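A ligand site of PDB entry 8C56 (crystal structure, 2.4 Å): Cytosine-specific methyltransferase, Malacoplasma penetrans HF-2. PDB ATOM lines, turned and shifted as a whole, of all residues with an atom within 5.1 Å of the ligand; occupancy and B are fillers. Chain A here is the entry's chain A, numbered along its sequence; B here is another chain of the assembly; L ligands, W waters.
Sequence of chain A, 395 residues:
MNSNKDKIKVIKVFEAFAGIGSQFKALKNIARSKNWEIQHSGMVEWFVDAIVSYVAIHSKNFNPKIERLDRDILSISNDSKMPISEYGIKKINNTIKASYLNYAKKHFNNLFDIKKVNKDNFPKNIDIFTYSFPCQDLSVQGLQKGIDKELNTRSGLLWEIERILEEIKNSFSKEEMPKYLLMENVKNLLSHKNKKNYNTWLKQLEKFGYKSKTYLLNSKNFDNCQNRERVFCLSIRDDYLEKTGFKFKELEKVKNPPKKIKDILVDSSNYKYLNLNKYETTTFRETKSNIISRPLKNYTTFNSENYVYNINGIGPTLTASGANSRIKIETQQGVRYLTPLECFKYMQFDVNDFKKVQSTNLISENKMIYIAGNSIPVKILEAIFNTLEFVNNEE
N of Ser 22 is in hydrogen-bond range of O1 of the ligand. O1 of the ligand lies within hydrogen-bond range of OG of Ser 22, at 2.6 Å. An oxygen (O5) of the ligand sits at hydrogen-bond distance from the side-chain carboxylate (OE2) of Glu 45 (2.7 Å). A nitrogen (N5) of the ligand is in hydrogen-bond range of the backbone NH (N) of Ile 114 (3.1 Å). The backbone NH (N) of Ile 20 sits at hydrogen-bond distance from an oxygen (O2) of the ligand (3.2 Å). N4 of the ligand sits at hydrogen-bond distance from OD1 of Asp 113 (3.2 Å). The indole nitrogen of Trp 46 lies within hydrogen-bond range of a nitrogen (N3) of the ligand. An oxygen (O1) of the ligand lies within hydrogen-bond range of the side-chain hydroxyl (OG) of Ser 375, at 3.4 Å. An oxygen (O1) of the ligand is in hydrogen-bond range of the backbone NH (N) of Gly 21, at 3.4 Å.
The backbone NH (N) of Glu 45 lies close to the backbone carbonyl oxygen (O) of Phe 112, 3.4 Å away. The backbone NH (N) of Gly 19 sits at hydrogen-bond distance from the side-chain carboxylate (OE1) of Glu 45 (2.7 Å). The backbone carbonyl oxygen (O) of Phe 112 is in hydrogen-bond range of the backbone NH (N) of Trp 46 (3.2 Å). O of Val 44 sits at hydrogen-bond distance from N of Ala 18, at 3.0 Å. N of Lys 115 lies close to OD1 of Asp 113, at 3.2 Å. NE1 of Trp 46 lies within hydrogen-bond range of O of Ser 80, 3.2 Å away. O of Val 44 is in hydrogen-bond range of N of Phe 17 (2.7 Å). The backbone carbonyl oxygen (O) of Ser 80 is in hydrogen-bond range of the guanidinium group (NH2) of Arg 154 (3.5 Å).
O1 of the ligand sits close to O of Ala 18, 3.1 Å away. O of Asn 374 sits close to S1 of the ligand. O of Phe 17 touches C3 of the ligand (3.3 Å). CA of Gly 19 touches O2 of the ligand, at 3.4 Å. Val 44 touches the ligand (CG1 to C13, 3.8 Å). Phe 47 touches the ligand. Ser 80 touches the ligand (CB to O5, 3.8 Å). Phe 112 touches the ligand. Ser 132 touches the ligand (O to C3, 3.2 Å). NH2 of Arg 154 touches C10 of the ligand, 3.7 Å away. CD1 of Leu 157 touches N3 of the ligand, 3.5 Å away. 5PY 8 of chain B touches the ligand. Within 4 Å of the ligand: Phe 17, Ala 18, Gly 19, Ile 20, Gly 21, Ser 22, Val 44, Glu 45, Trp 46, Phe 47, Ser 80, Phe 112, Asp 113, Ile 114, Ser 132, Arg 154, Leu 157, Asn 374, Ser 375 and 5PY 8 of chain B. The nearest printed residue that does not touch the ligand is Ile 376 (4.02 Å).
Water W2 bridges O2 of the ligand (2.6 Å) and O of Ile 371 (2.8 Å). Water W4 lies within hydrogen-bond range of O of Ala 18 (2.8 Å), N1 of the ligand (3.3 Å) and N of Gln 23 (3.3 Å).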
ATOM      1  N   PHE A  17      18.221   5.152 -23.344  1.00  0.00           N
ATOM      2  CA  PHE A  17      17.147   4.170 -23.281  1.00  0.00           C
ATOM      3  C   PHE A  17      16.078   4.527 -24.302  1.00  0.00           C
ATOM      4  O   PHE A  17      14.910   4.688 -23.971  1.00  0.00           O
ATOM      5  CB  PHE A  17      16.541   4.094 -21.887  1.00  0.00           C
ATOM      6  CG  PHE A  17      17.551   4.068 -20.780  1.00  0.00           C
ATOM      7  CD1 PHE A  17      18.284   2.924 -20.517  1.00  0.00           C
ATOM      8  CD2 PHE A  17      17.762   5.188 -19.987  1.00  0.00           C
ATOM      9  CE1 PHE A  17      19.209   2.902 -19.487  1.00  0.00           C
ATOM     10  CE2 PHE A  17      18.678   5.168 -18.946  1.00  0.00           C
ATOM     11  CZ  PHE A  17      19.405   4.019 -18.696  1.00  0.00           C
ATOM     12  N   ALA A  18      16.487   4.649 -25.560  1.00  0.00           N
ATOM     13  CA  ALA A  18      15.670   5.279 -26.586  1.00  0.00           C
ATOM     14  C   ALA A  18      14.401   4.506 -26.960  1.00  0.00           C
ATOM     15  O   ALA A  18      13.419   5.100 -27.387  1.00  0.00           O
ATOM     16  CB  ALA A  18      16.506   5.525 -27.842  1.00  0.00           C
ATOM     17  N   GLY A  19      14.452   3.184 -26.811  1.00  0.00           N
ATOM     18  CA  GLY A  19      13.341   2.326 -27.216  1.00  0.00           C
ATOM     19  C   GLY A  19      13.061   2.504 -28.694  1.00  0.00           C
ATOM     20  O   GLY A  19      13.990   2.436 -29.505  1.00  0.00           O
ATOM     21  N   ILE A  20      11.802   2.737 -29.041  1.00  0.00           N
ATOM     22  CA  ILE A  20      11.417   3.005 -30.430  1.00  0.00           C
ATOM     23  C   ILE A  20      11.344   4.495 -30.735  1.00  0.00           C
ATOM     24  O   ILE A  20      10.795   4.893 -31.772  1.00  0.00           O
ATOM     25  CB  ILE A  20      10.069   2.349 -30.811  1.00  0.00           C
ATOM     26  CG1 ILE A  20       8.906   2.977 -30.039  1.00  0.00           C
ATOM     27  CG2 ILE A  20      10.128   0.848 -30.577  1.00  0.00           C
ATOM     28  CD1 ILE A  20       7.580   2.269 -30.264  1.00  0.00           C
ATOM     29  N   GLY A  21      11.878   5.320 -29.842  1.00  0.00           N
ATOM     30  CA  GLY A  21      12.032   6.743 -30.101  1.00  0.00           C
ATOM     31  C   GLY A  21      10.758   7.558 -30.096  1.00  0.00           C
ATOM     32  O   GLY A  21      10.510   8.350 -31.001  1.00  0.00           O
ATOM     33  N   SER A  22       9.934   7.381 -29.073  1.00  0.00           N
ATOM     34  CA  SER A  22       8.788   8.260 -28.903  1.00  0.00           C
ATOM     35  C   SER A  22       9.224   9.712 -28.695  1.00  0.00           C
ATOM     36  O   SER A  22       8.521  10.619 -29.106  1.00  0.00           O
ATOM     37  CB  SER A  22       7.909   7.794 -27.737  1.00  0.00           C
ATOM     38  OG  SER A  22       8.704   7.496 -26.615  1.00  0.00           O
ATOM     39  N   GLN A  23      10.396   9.899 -28.086  1.00  0.00           N
ATOM     40  CA  GLN A  23      10.945  11.242 -27.857  1.00  0.00           C
ATOM     41  C   GLN A  23      11.262  11.907 -29.195  1.00  0.00           C
ATOM     42  O   GLN A  23      10.917  13.072 -29.417  1.00  0.00           O
ATOM     43  CB  GLN A  23      12.210  11.201 -26.995  1.00  0.00           C
ATOM     44  CG  GLN A  23      12.090  10.499 -25.642  1.00  0.00           C
ATOM     45  CD  GLN A  23      11.477  11.349 -24.551  1.00  0.00           C
ATOM     46  OE1 GLN A  23      11.044  12.475 -24.777  1.00  0.00           O
ATOM     47  NE2 GLN A  23      11.443  10.801 -23.339  1.00  0.00           N
ATOM     48  N   VAL A  44      21.039   5.584 -26.920  1.00  0.00           N
ATOM     49  CA  VAL A  44      21.472   4.395 -26.216  1.00  0.00           C
ATOM     50  C   VAL A  44      20.293   3.450 -26.079  1.00  0.00           C
ATOM     51  O   VAL A  44      19.305   3.755 -25.424  1.00  0.00           O
ATOM     52  CB  VAL A  44      22.002   4.702 -24.803  1.00  0.00           C
ATOM     53  CG1 VAL A  44      22.659   3.469 -24.215  1.00  0.00           C
ATOM     54  CG2 VAL A  44      22.972   5.871 -24.853  1.00  0.00           C
ATOM     55  N   GLU A  45      20.397   2.306 -26.759  1.00  0.00           N
ATOM     56  CA  GLU A  45      19.379   1.277 -26.688  1.00  0.00           C
ATOM     57  C   GLU A  45      20.022  -0.036 -27.074  1.00  0.00           C
ATOM     58  O   GLU A  45      20.621  -0.139 -28.141  1.00  0.00           O
ATOM     59  CB  GLU A  45      18.227   1.617 -27.641  1.00  0.00           C
ATOM     60  CG  GLU A  45      17.110   0.582 -27.655  1.00  0.00           C
ATOM     61  CD  GLU A  45      16.552   0.312 -26.278  1.00  0.00           C
ATOM     62  OE1 GLU A  45      16.000   1.263 -25.681  1.00  0.00           O
ATOM     63  OE2 GLU A  45      16.647  -0.827 -25.791  1.00  0.00           O
ATOM     64  N   TRP A  46      19.918  -1.018 -26.197  1.00  0.00           N
ATOM     65  CA  TRP A  46      20.583  -2.303 -26.400  1.00  0.00           C
ATOM     66  C   TRP A  46      19.642  -3.432 -26.792  1.00  0.00           C
ATOM     67  O   TRP A  46      20.088  -4.555 -27.011  1.00  0.00           O
ATOM     68  CB  TRP A  46      21.405  -2.685 -25.147  1.00  0.00           C
ATOM     69  CG  TRP A  46      20.656  -3.346 -24.025  1.00  0.00           C
ATOM     70  CD1 TRP A  46      19.360  -3.121 -23.645  1.00  0.00           C
ATOM     71  CD2 TRP A  46      21.183  -4.316 -23.099  1.00  0.00           C
ATOM     72  NE1 TRP A  46      19.045  -3.905 -22.550  1.00  0.00           N
ATOM     73  CE2 TRP A  46      20.140  -4.646 -22.201  1.00  0.00           C
ATOM     74  CE3 TRP A  46      22.425  -4.939 -22.947  1.00  0.00           C
ATOM     75  CZ2 TRP A  46      20.309  -5.577 -21.171  1.00  0.00           C
ATOM     76  CZ3 TRP A  46      22.593  -5.862 -21.927  1.00  0.00           C
ATOM     77  CH2 TRP A  46      21.543  -6.171 -21.058  1.00  0.00           C
ATOM     78  N   PHE A  47      18.343  -3.128 -26.877  1.00  0.00           N
ATOM     79  CA  PHE A  47      17.323  -4.136 -27.131  1.00  0.00           C
ATOM     80  C   PHE A  47      17.083  -4.302 -28.633  1.00  0.00           C
ATOM     81  O   PHE A  47      16.535  -3.423 -29.282  1.00  0.00           O
ATOM     82  CB  PHE A  47      16.050  -3.745 -26.380  1.00  0.00           C
ATOM     83  CG  PHE A  47      14.907  -4.712 -26.521  1.00  0.00           C
ATOM     84  CD1 PHE A  47      15.106  -6.086 -26.664  1.00  0.00           C
ATOM     85  CD2 PHE A  47      13.593  -4.231 -26.460  1.00  0.00           C
ATOM     86  CE1 PHE A  47      14.032  -6.946 -26.775  1.00  0.00           C
ATOM     87  CE2 PHE A  47      12.514  -5.104 -26.572  1.00  0.00           C
ATOM     88  CZ  PHE A  47      12.734  -6.462 -26.730  1.00  0.00           C
ATOM     89  N   ALA A  50      13.856  -3.320 -30.343  1.00  0.00           N
ATOM     90  CA  ALA A  50      13.654  -1.879 -30.256  1.00  0.00           C
ATOM     91  C   ALA A  50      14.572  -1.148 -31.225  1.00  0.00           C
ATOM     92  O   ALA A  50      14.155  -0.177 -31.875  1.00  0.00           O
ATOM     93  CB  ALA A  50      13.887  -1.382 -28.836  1.00  0.00           C
ATOM     94  N   SER A  80      15.778  -7.774 -23.665  1.00  0.00           N
ATOM     95  CA  SER A  80      15.832  -6.456 -23.004  1.00  0.00           C
ATOM     96  C   SER A  80      16.350  -6.470 -21.545  1.00  0.00           C
ATOM     97  O   SER A  80      16.633  -5.406 -20.992  1.00  0.00           O
ATOM     98  CB  SER A  80      14.495  -5.700 -23.089  1.00  0.00           C
ATOM     99  OG  SER A  80      13.622  -6.029 -22.014  1.00  0.00           O
ATOM    100  N   PHE A 112      24.467   1.900 -27.605  1.00  0.00           N
ATOM    101  CA  PHE A 112      23.924   0.600 -27.193  1.00  0.00           C
ATOM    102  C   PHE A 112      23.780   0.418 -25.689  1.00  0.00           C
ATOM    103  O   PHE A 112      22.655   0.294 -25.194  1.00  0.00           O
ATOM    104  CB  PHE A 112      24.733  -0.563 -27.795  1.00  0.00           C
ATOM    105  CG  PHE A 112      24.698  -0.607 -29.286  1.00  0.00           C
ATOM    106  CD1 PHE A 112      23.632  -1.186 -29.957  1.00  0.00           C
ATOM    107  CD2 PHE A 112      25.734  -0.057 -30.040  1.00  0.00           C
ATOM    108  CE1 PHE A 112      23.587  -1.227 -31.338  1.00  0.00           C
ATOM    109  CE2 PHE A 112      25.696  -0.093 -31.426  1.00  0.00           C
ATOM    110  CZ  PHE A 112      24.629  -0.681 -32.069  1.00  0.00           C
ATOM    111  N   ASP A 113      24.891   0.391 -24.968  1.00  0.00           N
ATOM    112  CA  ASP A 113      24.882   0.097 -23.532  1.00  0.00           C
ATOM    113  C   ASP A 113      25.254   1.357 -22.748  1.00  0.00           C
ATOM    114  O   ASP A 113      26.301   1.951 -22.977  1.00  0.00           O
ATOM    115  CB  ASP A 113      25.861  -1.037 -23.236  1.00  0.00           C
ATOM    116  CG  ASP A 113      25.837  -1.503 -21.782  1.00  0.00           C
ATOM    117  OD1 ASP A 113      25.053  -0.966 -20.959  1.00  0.00           O
ATOM    118  OD2 ASP A 113      26.620  -2.420 -21.451  1.00  0.00           O
ATOM    119  N   ILE A 114      24.387   1.725 -21.795  1.00  0.00           N
ATOM    120  CA  ILE A 114      24.550   2.942 -21.008  1.00  0.00           C
ATOM    121  C   ILE A 114      25.827   2.928 -20.162  1.00  0.00           C
ATOM    122  O   ILE A 114      26.400   3.978 -19.863  1.00  0.00           O
ATOM    123  CB  ILE A 114      23.316   3.197 -20.104  1.00  0.00           C
ATOM    124  CG1 ILE A 114      23.282   4.649 -19.607  1.00  0.00           C
ATOM    125  CG2 ILE A 114      23.278   2.216 -18.931  1.00  0.00           C
ATOM    126  CD1 ILE A 114      23.094   5.671 -20.710  1.00  0.00           C
ATOM    127  N   LYS A 115      26.280   1.722 -19.810  1.00  0.00           N
ATOM    128  CA  LYS A 115      27.544   1.518 -19.102  1.00  0.00           C
ATOM    129  C   LYS A 115      28.723   1.971 -19.941  1.00  0.00           C
ATOM    130  O   LYS A 115      29.725   2.418 -19.397  1.00  0.00           O
ATOM    131  CB  LYS A 115      27.734   0.039 -18.763  1.00  0.00           C
ATOM    132  CG  LYS A 115      26.602  -0.619 -17.994  1.00  0.00           C
ATOM    133  CD  LYS A 115      26.877  -0.659 -16.498  1.00  0.00           C
ATOM    134  CE  LYS A 115      25.854  -1.519 -15.770  1.00  0.00           C
ATOM    135  NZ  LYS A 115      26.001  -2.971 -16.090  1.00  0.00           N
ATOM    136  N   SER A 132      14.316   7.966 -20.387  1.00  0.00           N
ATOM    137  CA  SER A 132      13.237   7.121 -19.924  1.00  0.00           C
ATOM    138  C   SER A 132      13.839   5.790 -19.455  1.00  0.00           C
ATOM    139  O   SER A 132      13.798   4.793 -20.163  1.00  0.00           O
ATOM    140  CB  SER A 132      12.227   6.880 -21.050  1.00  0.00           C
ATOM    141  OG  SER A 132      11.220   5.963 -20.642  1.00  0.00           O
ATOM    142  N   PHE A 133      14.406   5.800 -18.246  1.00  0.00           N
ATOM    143  CA  PHE A 133      15.136   4.649 -17.711  1.00  0.00           C
ATOM    144  C   PHE A 133      14.197   3.481 -17.373  1.00  0.00           C
ATOM    145  O   PHE A 133      12.978   3.652 -17.366  1.00  0.00           O
ATOM    146  CB  PHE A 133      16.030   5.079 -16.528  1.00  0.00           C
ATOM    147  CG  PHE A 133      15.283   5.410 -15.265  1.00  0.00           C
ATOM    148  CD1 PHE A 133      14.795   6.697 -15.052  1.00  0.00           C
ATOM    149  CD2 PHE A 133      15.101   4.458 -14.283  1.00  0.00           C
ATOM    150  CE1 PHE A 133      14.109   7.011 -13.884  1.00  0.00           C
ATOM    151  CE2 PHE A 133      14.430   4.758 -13.108  1.00  0.00           C
ATOM    152  CZ  PHE A 133      13.930   6.044 -12.914  1.00  0.00           C
ATOM    153  N   PRO A 134      14.738   2.278 -17.119  1.00  0.00           N
ATOM    154  CA  PRO A 134      13.854   1.123 -16.933  1.00  0.00           C
ATOM    155  C   PRO A 134      12.888   1.276 -15.761  1.00  0.00           C
ATOM    156  O   PRO A 134      13.252   1.796 -14.701  1.00  0.00           O
ATOM    157  CB  PRO A 134      14.834  -0.037 -16.684  1.00  0.00           C
ATOM    158  CG  PRO A 134      16.076   0.377 -17.375  1.00  0.00           C
ATOM    159  CD  PRO A 134      16.161   1.863 -17.138  1.00  0.00           C
ATOM    160  N   ARG A 154      17.733  -2.992 -12.529  1.00  0.00           N
ATOM    161  CA  ARG A 154      17.662  -2.383 -13.863  1.00  0.00           C
ATOM    162  C   ARG A 154      17.142  -0.954 -13.809  1.00  0.00           C
ATOM    163  O   ARG A 154      17.641  -0.085 -14.535  1.00  0.00           O
ATOM    164  CB  ARG A 154      16.792  -3.226 -14.803  1.00  0.00           C
ATOM    165  CG  ARG A 154      17.356  -4.608 -15.089  1.00  0.00           C
ATOM    166  CD  ARG A 154      16.806  -5.177 -16.383  1.00  0.00           C
ATOM    167  NE  ARG A 154      15.360  -4.968 -16.532  1.00  0.00           N
ATOM    168  CZ  ARG A 154      14.818  -4.170 -17.439  1.00  0.00           C
ATOM    169  NH1 ARG A 154      13.491  -4.047 -17.513  1.00  0.00           N
ATOM    170  NH2 ARG A 154      15.574  -3.489 -18.286  1.00  0.00           N
ATOM    171  N   LEU A 157      19.725   1.678 -13.144  1.00  0.00           N
ATOM    172  CA  LEU A 157      20.548   2.236 -14.229  1.00  0.00           C
ATOM    173  C   LEU A 157      20.388   3.752 -14.325  1.00  0.00           C
ATOM    174  O   LEU A 157      21.182   4.411 -15.002  1.00  0.00           O
ATOM    175  CB  LEU A 157      20.221   1.571 -15.572  1.00  0.00           C
ATOM    176  CG  LEU A 157      20.651   0.108 -15.687  1.00  0.00           C
ATOM    177  CD1 LEU A 157      20.180  -0.508 -17.000  1.00  0.00           C
ATOM    178  CD2 LEU A 157      22.167  -0.029 -15.546  1.00  0.00           C
ATOM    179  N   ILE A 371       7.269  -3.583 -27.206  1.00  0.00           N
ATOM    180  CA  ILE A 371       7.982  -2.319 -27.396  1.00  0.00           C
ATOM    181  C   ILE A 371       7.058  -1.101 -27.323  1.00  0.00           C
ATOM    182  O   ILE A 371       7.462  -0.035 -26.842  1.00  0.00           O
ATOM    183  CB  ILE A 371       8.830  -2.289 -28.702  1.00  0.00           C
ATOM    184  CG1 ILE A 371       7.960  -2.415 -29.956  1.00  0.00           C
ATOM    185  CG2 ILE A 371       9.894  -3.388 -28.676  1.00  0.00           C
ATOM    186  CD1 ILE A 371       8.753  -2.720 -31.207  1.00  0.00           C
ATOM    187  N   ASN A 374       6.477  -0.530 -23.632  1.00  0.00           N
ATOM    188  CA  ASN A 374       7.649   0.112 -23.047  1.00  0.00           C
ATOM    189  C   ASN A 374       7.833   1.573 -23.447  1.00  0.00           C
ATOM    190  O   ASN A 374       8.749   2.221 -22.953  1.00  0.00           O
ATOM    191  CB  ASN A 374       8.922  -0.657 -23.410  1.00  0.00           C
ATOM    192  CG  ASN A 374       9.366  -1.607 -22.316  1.00  0.00           C
ATOM    193  OD1 ASN A 374       8.871  -1.575 -21.197  1.00  0.00           O
ATOM    194  ND2 ASN A 374      10.330  -2.451 -22.645  1.00  0.00           N
ATOM    195  N   SER A 375       6.984   2.111 -24.312  1.00  0.00           N
ATOM    196  CA  SER A 375       7.181   3.455 -24.839  1.00  0.00           C
ATOM    197  C   SER A 375       6.416   4.513 -24.023  1.00  0.00           C
ATOM    198  O   SER A 375       5.967   4.251 -22.909  1.00  0.00           O
ATOM    199  CB  SER A 375       6.762   3.483 -26.306  1.00  0.00           C
ATOM    200  OG  SER A 375       7.038   4.745 -26.888  1.00  0.00           O
ATOM    201  N   ILE A 376       6.290   5.717 -24.584  1.00  0.00           N
ATOM    202  CA  ILE A 376       5.611   6.838 -23.927  1.00  0.00           C
ATOM    203  C   ILE A 376       4.598   7.444 -24.890  1.00  0.00           C
ATOM    204  O   ILE A 376       4.934   7.672 -26.056  1.00  0.00           O
ATOM    205  CB  ILE A 376       6.611   7.950 -23.530  1.00  0.00           C
ATOM    206  CG1 ILE A 376       7.702   7.394 -22.628  1.00  0.00           C
ATOM    207  CG2 ILE A 376       5.896   9.098 -22.834  1.00  0.00           C
ATOM    208  CD1 ILE A 376       8.933   8.285 -22.548  1.00  0.00           C
ATOM    209  P   5PY B   8       2.623   0.538 -14.688  1.00  0.00           P
ATOM    210  OP2 5PY B   8       1.854   1.797 -14.960  1.00  0.00           O
ATOM    211  OP1 5PY B   8       3.795   0.552 -13.756  1.00  0.00           O
ATOM    212  O5' 5PY B   8       3.108  -0.033 -16.107  1.00  0.00           O
ATOM    213  C5' 5PY B   8       4.248  -0.862 -16.194  1.00  0.00           C
ATOM    214  C4' 5PY B   8       4.733  -0.711 -17.619  1.00  0.00           C
ATOM    215  O4' 5PY B   8       5.319   0.571 -17.865  1.00  0.00           O
ATOM    216  C1' 5PY B   8       6.113   0.429 -19.045  1.00  0.00           C
ATOM    217  N1  5PY B   8       7.259   1.360 -19.040  1.00  0.00           N
ATOM    218  C2  5PY B   8       6.997   2.756 -18.942  1.00  0.00           C
ATOM    219  O2  5PY B   8       5.832   3.166 -18.848  1.00  0.00           O
ATOM    220  N3  5PY B   8       8.008   3.674 -18.937  1.00  0.00           N
ATOM    221  C4  5PY B   8       9.295   3.277 -19.048  1.00  0.00           C
ATOM    222  C5  5PY B   8       9.594   1.829 -19.169  1.00  0.00           C
ATOM    223  C5M 5PY B   8      10.999   1.318 -19.316  1.00  0.00           C
ATOM    224  C6  5PY B   8       8.543   0.935 -19.164  1.00  0.00           C
ATOM    225  C2' 5PY B   8       6.462  -1.070 -19.169  1.00  0.00           C
ATOM    226  C3' 5PY B   8       5.781  -1.732 -17.996  1.00  0.00           C
ATOM    227  O3' 5PY B   8       5.166  -2.958 -18.376  1.00  0.00           O
HETATM  228  N1  LIG L   1      11.709   6.050 -24.413  1.00  0.00           N
HETATM  229  C1  LIG L   1      11.562   4.620 -24.838  1.00  0.00           C
HETATM  230  C2  LIG L   1      11.054   3.815 -23.634  1.00  0.00           C
HETATM  231  C3  LIG L   1      12.116   3.570 -22.544  1.00  0.00           C
HETATM  232  S1  LIG L   1      12.264   1.826 -22.321  1.00  0.00           S
HETATM  233  C4  LIG L   1      10.647   4.486 -26.061  1.00  0.00           C
HETATM  234  O1  LIG L   1      10.361   5.440 -26.787  1.00  0.00           O
HETATM  235  O2  LIG L   1      10.168   3.410 -26.416  1.00  0.00           O
HETATM  236  C5  LIG L   1      13.756   1.505 -21.436  1.00  0.00           C
HETATM  237  C6  LIG L   1      14.767   0.855 -22.384  1.00  0.00           C
HETATM  238  O3  LIG L   1      16.056   0.732 -21.757  1.00  0.00           O
HETATM  239  C7  LIG L   1      14.398  -0.549 -22.851  1.00  0.00           C
HETATM  240  O4  LIG L   1      14.044  -0.586 -24.235  1.00  0.00           O
HETATM  241  C8  LIG L   1      15.641  -1.383 -22.575  1.00  0.00           C
HETATM  242  O5  LIG L   1      15.919  -2.257 -23.656  1.00  0.00           O
HETATM  243  C9  LIG L   1      16.754  -0.348 -22.365  1.00  0.00           C
HETATM  244  N2  LIG L   1      17.915  -0.825 -21.545  1.00  0.00           N
HETATM  245  C10 LIG L   1      17.834  -1.662 -20.502  1.00  0.00           C
HETATM  246  N3  LIG L   1      19.056  -1.927 -19.957  1.00  0.00           N
HETATM  247  C11 LIG L   1      19.956  -1.233 -20.669  1.00  0.00           C
HETATM  248  C12 LIG L   1      21.426  -1.059 -20.627  1.00  0.00           C
HETATM  249  N4  LIG L   1      22.181  -1.694 -19.693  1.00  0.00           N
HETATM  250  N5  LIG L   1      21.971  -0.247 -21.549  1.00  0.00           N
HETATM  251  C13 LIG L   1      21.225   0.377 -22.482  1.00  0.00           C
HETATM  252  N6  LIG L   1      19.880   0.271 -22.581  1.00  0.00           N
HETATM  253  C14 LIG L   1      19.200  -0.511 -21.715  1.00  0.00           C
HETATM  254  O   HOH W   1      11.779  -1.340 -25.703  1.00  0.00           O
HETATM  255  O   HOH W   2      10.124   0.842 -26.586  1.00  0.00           O
HETATM  256  O   HOH W   3      13.512  -1.713 -20.008  1.00  0.00           O
HETATM  257  O   HOH W   4      12.774   7.846 -26.983  1.00  0.00           O
